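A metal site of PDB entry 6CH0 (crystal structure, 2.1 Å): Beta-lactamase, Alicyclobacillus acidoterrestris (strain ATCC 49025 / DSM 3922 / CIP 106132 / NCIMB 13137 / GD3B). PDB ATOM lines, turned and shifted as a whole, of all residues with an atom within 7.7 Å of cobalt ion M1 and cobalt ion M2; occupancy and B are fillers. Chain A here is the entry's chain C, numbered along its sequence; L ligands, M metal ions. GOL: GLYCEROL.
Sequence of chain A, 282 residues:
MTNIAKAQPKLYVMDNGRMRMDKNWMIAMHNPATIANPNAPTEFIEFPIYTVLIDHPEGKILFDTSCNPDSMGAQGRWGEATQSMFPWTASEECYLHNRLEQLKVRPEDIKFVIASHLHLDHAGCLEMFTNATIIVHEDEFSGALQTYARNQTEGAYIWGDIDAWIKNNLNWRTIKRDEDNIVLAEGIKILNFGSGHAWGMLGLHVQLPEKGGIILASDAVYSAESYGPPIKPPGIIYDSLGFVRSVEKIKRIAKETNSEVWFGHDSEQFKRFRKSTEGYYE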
ATOM      1  N   MET A  19     -19.942   2.423  34.745  1.00  0.00           N
ATOM      2  CA  MET A  19     -20.815   2.573  33.606  1.00  0.00           C
ATOM      3  C   MET A  19     -21.088   1.173  33.088  1.00  0.00           C
ATOM      4  O   MET A  19     -20.294   0.265  33.330  1.00  0.00           O
ATOM      5  CB  MET A  19     -20.136   3.432  32.534  1.00  0.00           C
ATOM      6  CG  MET A  19     -20.941   3.620  31.260  1.00  0.00           C
ATOM      7  SD  MET A  19     -20.211   4.827  30.117  1.00  0.00           S
ATOM      8  CE  MET A  19     -20.471   6.364  30.980  1.00  0.00           C
ATOM      9  N   MET A  21     -22.550  -0.979  29.451  1.00  0.00           N
ATOM     10  CA  MET A  21     -22.950  -0.900  28.051  1.00  0.00           C
ATOM     11  C   MET A  21     -22.845  -2.252  27.385  1.00  0.00           C
ATOM     12  O   MET A  21     -22.237  -3.176  27.928  1.00  0.00           O
ATOM     13  CB  MET A  21     -22.065   0.095  27.296  1.00  0.00           C
ATOM     14  CG  MET A  21     -20.653  -0.416  27.063  1.00  0.00           C
ATOM     15  SD  MET A  21     -19.566   0.900  26.487  1.00  0.00           S
ATOM     16  CE  MET A  21     -17.980   0.085  26.659  1.00  0.00           C
ATOM     17  N   PHE A  47     -17.950  -1.345  33.841  1.00  0.00           N
ATOM     18  CA  PHE A  47     -16.540  -0.971  33.877  1.00  0.00           C
ATOM     19  C   PHE A  47     -16.335   0.351  34.607  1.00  0.00           C
ATOM     20  O   PHE A  47     -17.228   1.162  34.694  1.00  0.00           O
ATOM     21  CB  PHE A  47     -15.982  -0.909  32.462  1.00  0.00           C
ATOM     22  CG  PHE A  47     -16.748   0.010  31.565  1.00  0.00           C
ATOM     23  CD1 PHE A  47     -16.425   1.350  31.484  1.00  0.00           C
ATOM     24  CD2 PHE A  47     -17.797  -0.468  30.802  1.00  0.00           C
ATOM     25  CE1 PHE A  47     -17.126   2.199  30.663  1.00  0.00           C
ATOM     26  CE2 PHE A  47     -18.512   0.380  29.982  1.00  0.00           C
ATOM     27  CZ  PHE A  47     -18.174   1.715  29.906  1.00  0.00           C
ATOM     28  N   PRO A  48     -15.134   0.561  35.145  1.00  0.00           N
ATOM     29  CA  PRO A  48     -14.912   1.751  35.923  1.00  0.00           C
ATOM     30  C   PRO A  48     -14.669   2.983  35.056  1.00  0.00           C
ATOM     31  O   PRO A  48     -14.155   2.873  33.952  1.00  0.00           O
ATOM     32  CB  PRO A  48     -13.658   1.412  36.709  1.00  0.00           C
ATOM     33  CG  PRO A  48     -12.888   0.562  35.771  1.00  0.00           C
ATOM     34  CD  PRO A  48     -13.909  -0.246  35.021  1.00  0.00           C
ATOM     35  N   ILE A  49     -15.070   4.133  35.586  1.00  0.00           N
ATOM     36  CA  ILE A  49     -14.712   5.426  35.051  1.00  0.00           C
ATOM     37  C   ILE A  49     -13.774   6.002  36.073  1.00  0.00           C
ATOM     38  O   ILE A  49     -14.071   5.963  37.268  1.00  0.00           O
ATOM     39  CB  ILE A  49     -15.925   6.368  35.007  1.00  0.00           C
ATOM     40  CG1 ILE A  49     -17.036   5.800  34.117  1.00  0.00           C
ATOM     41  CG2 ILE A  49     -15.527   7.758  34.536  1.00  0.00           C
ATOM     42  CD1 ILE A  49     -16.590   5.551  32.706  1.00  0.00           C
ATOM     43  N   ASP A  64      -8.028  13.554  32.460  1.00  0.00           N
ATOM     44  CA  ASP A  64      -9.460  13.256  32.361  1.00  0.00           C
ATOM     45  C   ASP A  64     -10.275  13.853  33.512  1.00  0.00           C
ATOM     46  O   ASP A  64      -9.717  14.330  34.497  1.00  0.00           O
ATOM     47  CB  ASP A  64      -9.712  11.744  32.205  1.00  0.00           C
ATOM     48  CG  ASP A  64      -9.490  11.266  30.762  1.00  0.00           C
ATOM     49  OD1 ASP A  64      -9.380  12.135  29.863  1.00  0.00           O
ATOM     50  OD2 ASP A  64      -9.415  10.033  30.520  1.00  0.00           O
ATOM     51  N   SER A 116      -8.166  13.644  27.440  1.00  0.00           N
ATOM     52  CA  SER A 116      -7.772  12.581  26.533  1.00  0.00           C
ATOM     53  C   SER A 116      -8.540  12.723  25.233  1.00  0.00           C
ATOM     54  O   SER A 116      -7.986  12.590  24.141  1.00  0.00           O
ATOM     55  CB  SER A 116      -8.051  11.210  27.131  1.00  0.00           C
ATOM     56  OG  SER A 116      -9.444  10.987  27.264  1.00  0.00           O
ATOM     57  N   HIS A 117      -9.831  13.007  25.379  1.00  0.00           N
ATOM     58  CA  HIS A 117     -10.717  13.316  24.264  1.00  0.00           C
ATOM     59  C   HIS A 117     -11.981  13.907  24.888  1.00  0.00           C
ATOM     60  O   HIS A 117     -12.014  14.100  26.093  1.00  0.00           O
ATOM     61  CB  HIS A 117     -10.974  12.084  23.390  1.00  0.00           C
ATOM     62  CG  HIS A 117     -11.614  10.931  24.088  1.00  0.00           C
ATOM     63  ND1 HIS A 117     -11.123  10.415  25.259  1.00  0.00           N
ATOM     64  CD2 HIS A 117     -12.705  10.196  23.766  1.00  0.00           C
ATOM     65  CE1 HIS A 117     -11.875   9.390  25.631  1.00  0.00           C
ATOM     66  NE2 HIS A 117     -12.834   9.241  24.739  1.00  0.00           N
ATOM     67  N   LEU A 118     -12.993  14.248  24.096  1.00  0.00           N
ATOM     68  CA  LEU A 118     -14.121  15.038  24.636  1.00  0.00           C
ATOM     69  C   LEU A 118     -15.412  14.252  24.728  1.00  0.00           C
ATOM     70  O   LEU A 118     -16.509  14.813  24.685  1.00  0.00           O
ATOM     71  CB  LEU A 118     -14.322  16.336  23.830  1.00  0.00           C
ATOM     72  CG  LEU A 118     -13.072  17.211  23.898  1.00  0.00           C
ATOM     73  CD1 LEU A 118     -13.188  18.432  23.007  1.00  0.00           C
ATOM     74  CD2 LEU A 118     -12.813  17.596  25.346  1.00  0.00           C
ATOM     75  N   HIS A 119     -15.300  12.949  24.905  1.00  0.00           N
ATOM     76  CA  HIS A 119     -16.464  12.139  25.164  1.00  0.00           C
ATOM     77  C   HIS A 119     -17.050  12.354  26.569  1.00  0.00           C
ATOM     78  O   HIS A 119     -16.404  12.933  27.465  1.00  0.00           O
ATOM     79  CB  HIS A 119     -16.132  10.673  25.035  1.00  0.00           C
ATOM     80  CG  HIS A 119     -16.119  10.177  23.631  1.00  0.00           C
ATOM     81  ND1 HIS A 119     -15.477   9.007  23.264  1.00  0.00           N
ATOM     82  CD2 HIS A 119     -16.654  10.681  22.501  1.00  0.00           C
ATOM     83  CE1 HIS A 119     -15.654   8.811  21.967  1.00  0.00           C
ATOM     84  NE2 HIS A 119     -16.355   9.811  21.480  1.00  0.00           N
ATOM     85  N   LEU A 120     -18.268  11.839  26.724  1.00  0.00           N
ATOM     86  CA  LEU A 120     -19.118  12.067  27.876  1.00  0.00           C
ATOM     87  C   LEU A 120     -18.529  11.592  29.202  1.00  0.00           C
ATOM     88  O   LEU A 120     -18.786  12.203  30.235  1.00  0.00           O
ATOM     89  CB  LEU A 120     -20.493  11.411  27.639  1.00  0.00           C
ATOM     90  CG  LEU A 120     -20.688   9.898  27.688  1.00  0.00           C
ATOM     91  CD1 LEU A 120     -22.137   9.551  27.381  1.00  0.00           C
ATOM     92  CD2 LEU A 120     -19.784   9.136  26.742  1.00  0.00           C
ATOM     93  N   ASP A 121     -17.741  10.522  29.158  1.00  0.00           N
ATOM     94  CA  ASP A 121     -17.147   9.936  30.365  1.00  0.00           C
ATOM     95  C   ASP A 121     -15.727  10.408  30.650  1.00  0.00           C
ATOM     96  O   ASP A 121     -15.093   9.916  31.581  1.00  0.00           O
ATOM     97  CB  ASP A 121     -17.141   8.418  30.279  1.00  0.00           C
ATOM     98  CG  ASP A 121     -16.523   7.918  28.979  1.00  0.00           C
ATOM     99  OD1 ASP A 121     -16.863   8.476  27.923  1.00  0.00           O
ATOM    100  OD2 ASP A 121     -15.711   6.970  29.014  1.00  0.00           O
ATOM    101  N   HIS A 122     -15.203  11.345  29.867  1.00  0.00           N
ATOM    102  CA  HIS A 122     -13.862  11.892  30.159  1.00  0.00           C
ATOM    103  C   HIS A 122     -13.853  13.411  30.243  1.00  0.00           C
ATOM    104  O   HIS A 122     -12.979  13.996  30.877  1.00  0.00           O
ATOM    105  CB  HIS A 122     -12.843  11.403  29.137  1.00  0.00           C
ATOM    106  CG  HIS A 122     -12.725   9.916  29.059  1.00  0.00           C
ATOM    107  ND1 HIS A 122     -11.748   9.214  29.728  1.00  0.00           N
ATOM    108  CD2 HIS A 122     -13.481   8.988  28.420  1.00  0.00           C
ATOM    109  CE1 HIS A 122     -11.896   7.922  29.486  1.00  0.00           C
ATOM    110  NE2 HIS A 122     -12.936   7.757  28.698  1.00  0.00           N
ATOM    111  N   GLU A 140     -10.144  17.085  17.814  1.00  0.00           N
ATOM    112  CA  GLU A 140     -11.163  16.643  18.766  1.00  0.00           C
ATOM    113  C   GLU A 140     -12.007  17.837  19.201  1.00  0.00           C
ATOM    114  O   GLU A 140     -13.222  17.765  19.265  1.00  0.00           O
ATOM    115  CB  GLU A 140     -10.494  15.945  19.972  1.00  0.00           C
ATOM    116  CG  GLU A 140     -11.447  15.346  20.996  1.00  0.00           C
ATOM    117  CD  GLU A 140     -12.244  14.158  20.458  1.00  0.00           C
ATOM    118  OE1 GLU A 140     -11.908  13.635  19.369  1.00  0.00           O
ATOM    119  OE2 GLU A 140     -13.212  13.755  21.119  1.00  0.00           O
ATOM    120  N   ALA A 156     -22.190  10.634  22.008  1.00  0.00           N
ATOM    121  CA  ALA A 156     -21.121  10.582  23.002  1.00  0.00           C
ATOM    122  C   ALA A 156     -20.551  11.955  23.327  1.00  0.00           C
ATOM    123  O   ALA A 156     -19.752  12.102  24.252  1.00  0.00           O
ATOM    124  CB  ALA A 156     -20.013   9.651  22.538  1.00  0.00           C
ATOM    125  N   TYR A 157     -20.962  12.959  22.549  1.00  0.00           N
ATOM    126  CA  TYR A 157     -20.601  14.348  22.803  1.00  0.00           C
ATOM    127  C   TYR A 157     -21.826  15.070  23.380  1.00  0.00           C
ATOM    128  O   TYR A 157     -22.847  15.170  22.749  1.00  0.00           O
ATOM    129  CB  TYR A 157     -20.089  14.995  21.514  1.00  0.00           C
ATOM    130  CG  TYR A 157     -18.780  14.365  21.073  1.00  0.00           C
ATOM    131  CD1 TYR A 157     -17.566  14.812  21.609  1.00  0.00           C
ATOM    132  CD2 TYR A 157     -18.751  13.273  20.199  1.00  0.00           C
ATOM    133  CE1 TYR A 157     -16.370  14.236  21.235  1.00  0.00           C
ATOM    134  CE2 TYR A 157     -17.546  12.686  19.826  1.00  0.00           C
ATOM    135  CZ  TYR A 157     -16.359  13.174  20.352  1.00  0.00           C
ATOM    136  OH  TYR A 157     -15.160  12.613  20.023  1.00  0.00           O
ATOM    137  N   HIS A 197     -10.044   6.020  18.042  1.00  0.00           N
ATOM    138  CA  HIS A 197     -11.265   5.907  18.811  1.00  0.00           C
ATOM    139  C   HIS A 197     -12.127   7.174  18.609  1.00  0.00           C
ATOM    140  O   HIS A 197     -13.346   7.097  18.433  1.00  0.00           O
ATOM    141  CB  HIS A 197     -10.905   5.663  20.281  1.00  0.00           C
ATOM    142  CG  HIS A 197     -12.033   5.880  21.231  1.00  0.00           C
ATOM    143  ND1 HIS A 197     -13.102   5.031  21.341  1.00  0.00           N
ATOM    144  CD2 HIS A 197     -12.247   6.866  22.150  1.00  0.00           C
ATOM    145  CE1 HIS A 197     -13.935   5.480  22.252  1.00  0.00           C
ATOM    146  NE2 HIS A 197     -13.439   6.584  22.766  1.00  0.00           N
ATOM    147  N   ALA A 198     -11.464   8.331  18.600  1.00  0.00           N
ATOM    148  CA  ALA A 198     -12.150   9.596  18.300  1.00  0.00           C
ATOM    149  C   ALA A 198     -11.292  10.449  17.359  1.00  0.00           C
ATOM    150  O   ALA A 198     -10.295   9.968  16.819  1.00  0.00           O
ATOM    151  CB  ALA A 198     -12.450  10.330  19.588  1.00  0.00           C
ATOM    152  N   MET A 201      -6.974  11.780  20.014  1.00  0.00           N
ATOM    153  CA  MET A 201      -6.718  11.173  21.315  1.00  0.00           C
ATOM    154  C   MET A 201      -5.363  11.585  21.872  1.00  0.00           C
ATOM    155  O   MET A 201      -4.352  11.454  21.184  1.00  0.00           O
ATOM    156  CB  MET A 201      -6.713   9.667  21.168  1.00  0.00           C
ATOM    157  CG  MET A 201      -7.963   9.104  20.519  1.00  0.00           C
ATOM    158  SD  MET A 201      -9.410   9.270  21.570  1.00  0.00           S
ATOM    159  CE  MET A 201      -8.923   8.417  23.063  1.00  0.00           C
ATOM    160  N   SER A 218      -6.255   6.005  28.334  1.00  0.00           N
ATOM    161  CA  SER A 218      -7.643   6.379  28.199  1.00  0.00           C
ATOM    162  C   SER A 218      -8.320   5.466  27.163  1.00  0.00           C
ATOM    163  O   SER A 218      -8.029   4.286  27.123  1.00  0.00           O
ATOM    164  CB  SER A 218      -7.779   7.850  27.824  1.00  0.00           C
ATOM    165  OG  SER A 218      -9.144   8.221  27.769  1.00  0.00           O
ATOM    166  N   ASP A 219      -9.206   6.011  26.341  1.00  0.00           N
ATOM    167  CA  ASP A 219      -9.974   5.189  25.405  1.00  0.00           C
ATOM    168  C   ASP A 219      -9.197   4.742  24.170  1.00  0.00           C
ATOM    169  O   ASP A 219      -9.754   4.082  23.301  1.00  0.00           O
ATOM    170  CB  ASP A 219     -11.220   5.911  24.916  1.00  0.00           C
ATOM    171  CG  ASP A 219     -12.318   6.000  25.959  1.00  0.00           C
ATOM    172  OD1 ASP A 219     -12.217   5.328  27.020  1.00  0.00           O
ATOM    173  OD2 ASP A 219     -13.291   6.749  25.706  1.00  0.00           O
ATOM    174  N   ALA A 220      -7.914   5.108  24.079  1.00  0.00           N
ATOM    175  CA  ALA A 220      -7.088   4.570  23.017  1.00  0.00           C
ATOM    176  C   ALA A 220      -6.949   3.058  23.188  1.00  0.00           C
ATOM    177  O   ALA A 220      -6.761   2.348  22.212  1.00  0.00           O
ATOM    178  CB  ALA A 220      -5.723   5.249  22.988  1.00  0.00           C
ATOM    179  N   TYR A 222      -9.242   0.282  25.563  1.00  0.00           N
ATOM    180  CA  TYR A 222     -10.275   0.117  26.575  1.00  0.00           C
ATOM    181  C   TYR A 222      -9.813  -0.812  27.700  1.00  0.00           C
ATOM    182  O   TYR A 222     -10.050  -0.535  28.876  1.00  0.00           O
ATOM    183  CB  TYR A 222     -11.539  -0.489  25.956  1.00  0.00           C
ATOM    184  CG  TYR A 222     -12.536   0.457  25.329  1.00  0.00           C
ATOM    185  CD1 TYR A 222     -12.683   1.769  25.770  1.00  0.00           C
ATOM    186  CD2 TYR A 222     -13.385   0.019  24.330  1.00  0.00           C
ATOM    187  CE1 TYR A 222     -13.627   2.611  25.212  1.00  0.00           C
ATOM    188  CE2 TYR A 222     -14.322   0.857  23.766  1.00  0.00           C
ATOM    189  CZ  TYR A 222     -14.438   2.147  24.208  1.00  0.00           C
ATOM    190  OH  TYR A 222     -15.395   2.951  23.628  1.00  0.00           O
ATOM    191  N   GLY A 264      -8.179   2.561  29.798  1.00  0.00           N
ATOM    192  CA  GLY A 264      -9.261   3.465  30.141  1.00  0.00           C
ATOM    193  C   GLY A 264     -10.313   2.825  31.009  1.00  0.00           C
ATOM    194  O   GLY A 264     -10.799   3.459  31.925  1.00  0.00           O
ATOM    195  N   HIS A 265     -10.666   1.563  30.741  1.00  0.00           N
ATOM    196  CA  HIS A 265     -11.849   0.954  31.347  1.00  0.00           C
ATOM    197  C   HIS A 265     -11.735  -0.560  31.609  1.00  0.00           C
ATOM    198  O   HIS A 265     -12.646  -1.304  31.284  1.00  0.00           O
ATOM    199  CB  HIS A 265     -13.055   1.195  30.448  1.00  0.00           C
ATOM    200  CG  HIS A 265     -13.370   2.635  30.240  1.00  0.00           C
ATOM    201  ND1 HIS A 265     -13.631   3.499  31.275  1.00  0.00           N
ATOM    202  CD2 HIS A 265     -13.486   3.369  29.100  1.00  0.00           C
ATOM    203  CE1 HIS A 265     -13.874   4.706  30.791  1.00  0.00           C
ATOM    204  NE2 HIS A 265     -13.781   4.654  29.471  1.00  0.00           N
HETATM  205  C1  GOL L   1     -17.711   4.970  26.764  1.00  0.00           C
HETATM  206  O1  GOL L   1     -18.639   5.011  25.670  1.00  0.00           O
HETATM  207  C2  GOL L   1     -16.326   4.746  26.208  1.00  0.00           C
HETATM  208  O2  GOL L   1     -15.418   4.961  27.282  1.00  0.00           O
HETATM  209  C3  GOL L   1     -16.009   5.662  25.007  1.00  0.00           C
HETATM  210  O3  GOL L   1     -15.802   7.043  25.358  1.00  0.00           O
HETATM  211 CO    CO M   1     -14.286   7.736  24.404  1.00  0.00          CO
HETATM  212 CO    CO M   2     -14.175   6.186  28.013  1.00  0.00          CO
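A ring nitrogen (ND1) of His 265 is in hydrogen-bond range of the backbone carbonyl oxygen (O) of Pro 48 (2.8 Å).
A ring nitrogen (ND1) of His 122 lies within hydrogen-bond range of the side-chain carboxylate (OD2) of Asp 64 (2.6 Å).
O of Tyr 222 is in hydrogen-bond range of N of His 265 (2.9 Å).
ND1 of His 117 is in hydrogen-bond range of OG of Ser 116 (2.7 Å).
A ring nitrogen (ND1) of His 122 sits close to the side-chain hydroxyl (OG) of Ser 218 (3.4 Å).
A ring nitrogen (NE2) of His 119 lies within hydrogen-bond range of the side-chain hydroxyl (OH) of Tyr 157 (3.4 Å).
Along chain A the residues within 4 Å of cobalt ion M1 span positions 117 to 219.
Of the 25 residues printed, 4 come within 4 Å of cobalt ion M2.
The nearest printed residue that does not touch cobalt ion M2 is Tyr 222 (4.6 Å).
Cobalt ion M1 is bound by OD2 of Asp 219 (1.9 Å), O3 of the ligand (1.9 Å), ND1 of His 119 (2.1 Å), NE2 of His 117 (2.1 Å) and NE2 of His 197 (2.2 Å).
Cobalt ion M2 is bound by an oxygen (O2) of the ligand (1.9 Å), the side-chain carboxylate (OD2) of Asp 121 (2.0 Å), a ring nitrogen (NE2) of His 122 (2.1 Å), a ring nitrogen (NE2) of His 265 (2.2 Å), the side-chain carboxylate (OD1) of Asp 219 (2.4 Å) and the side-chain carboxylate (OD2) of Asp 219 (2.5 Å).
Cobalt ion M2 has six donor atoms within binding distance.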
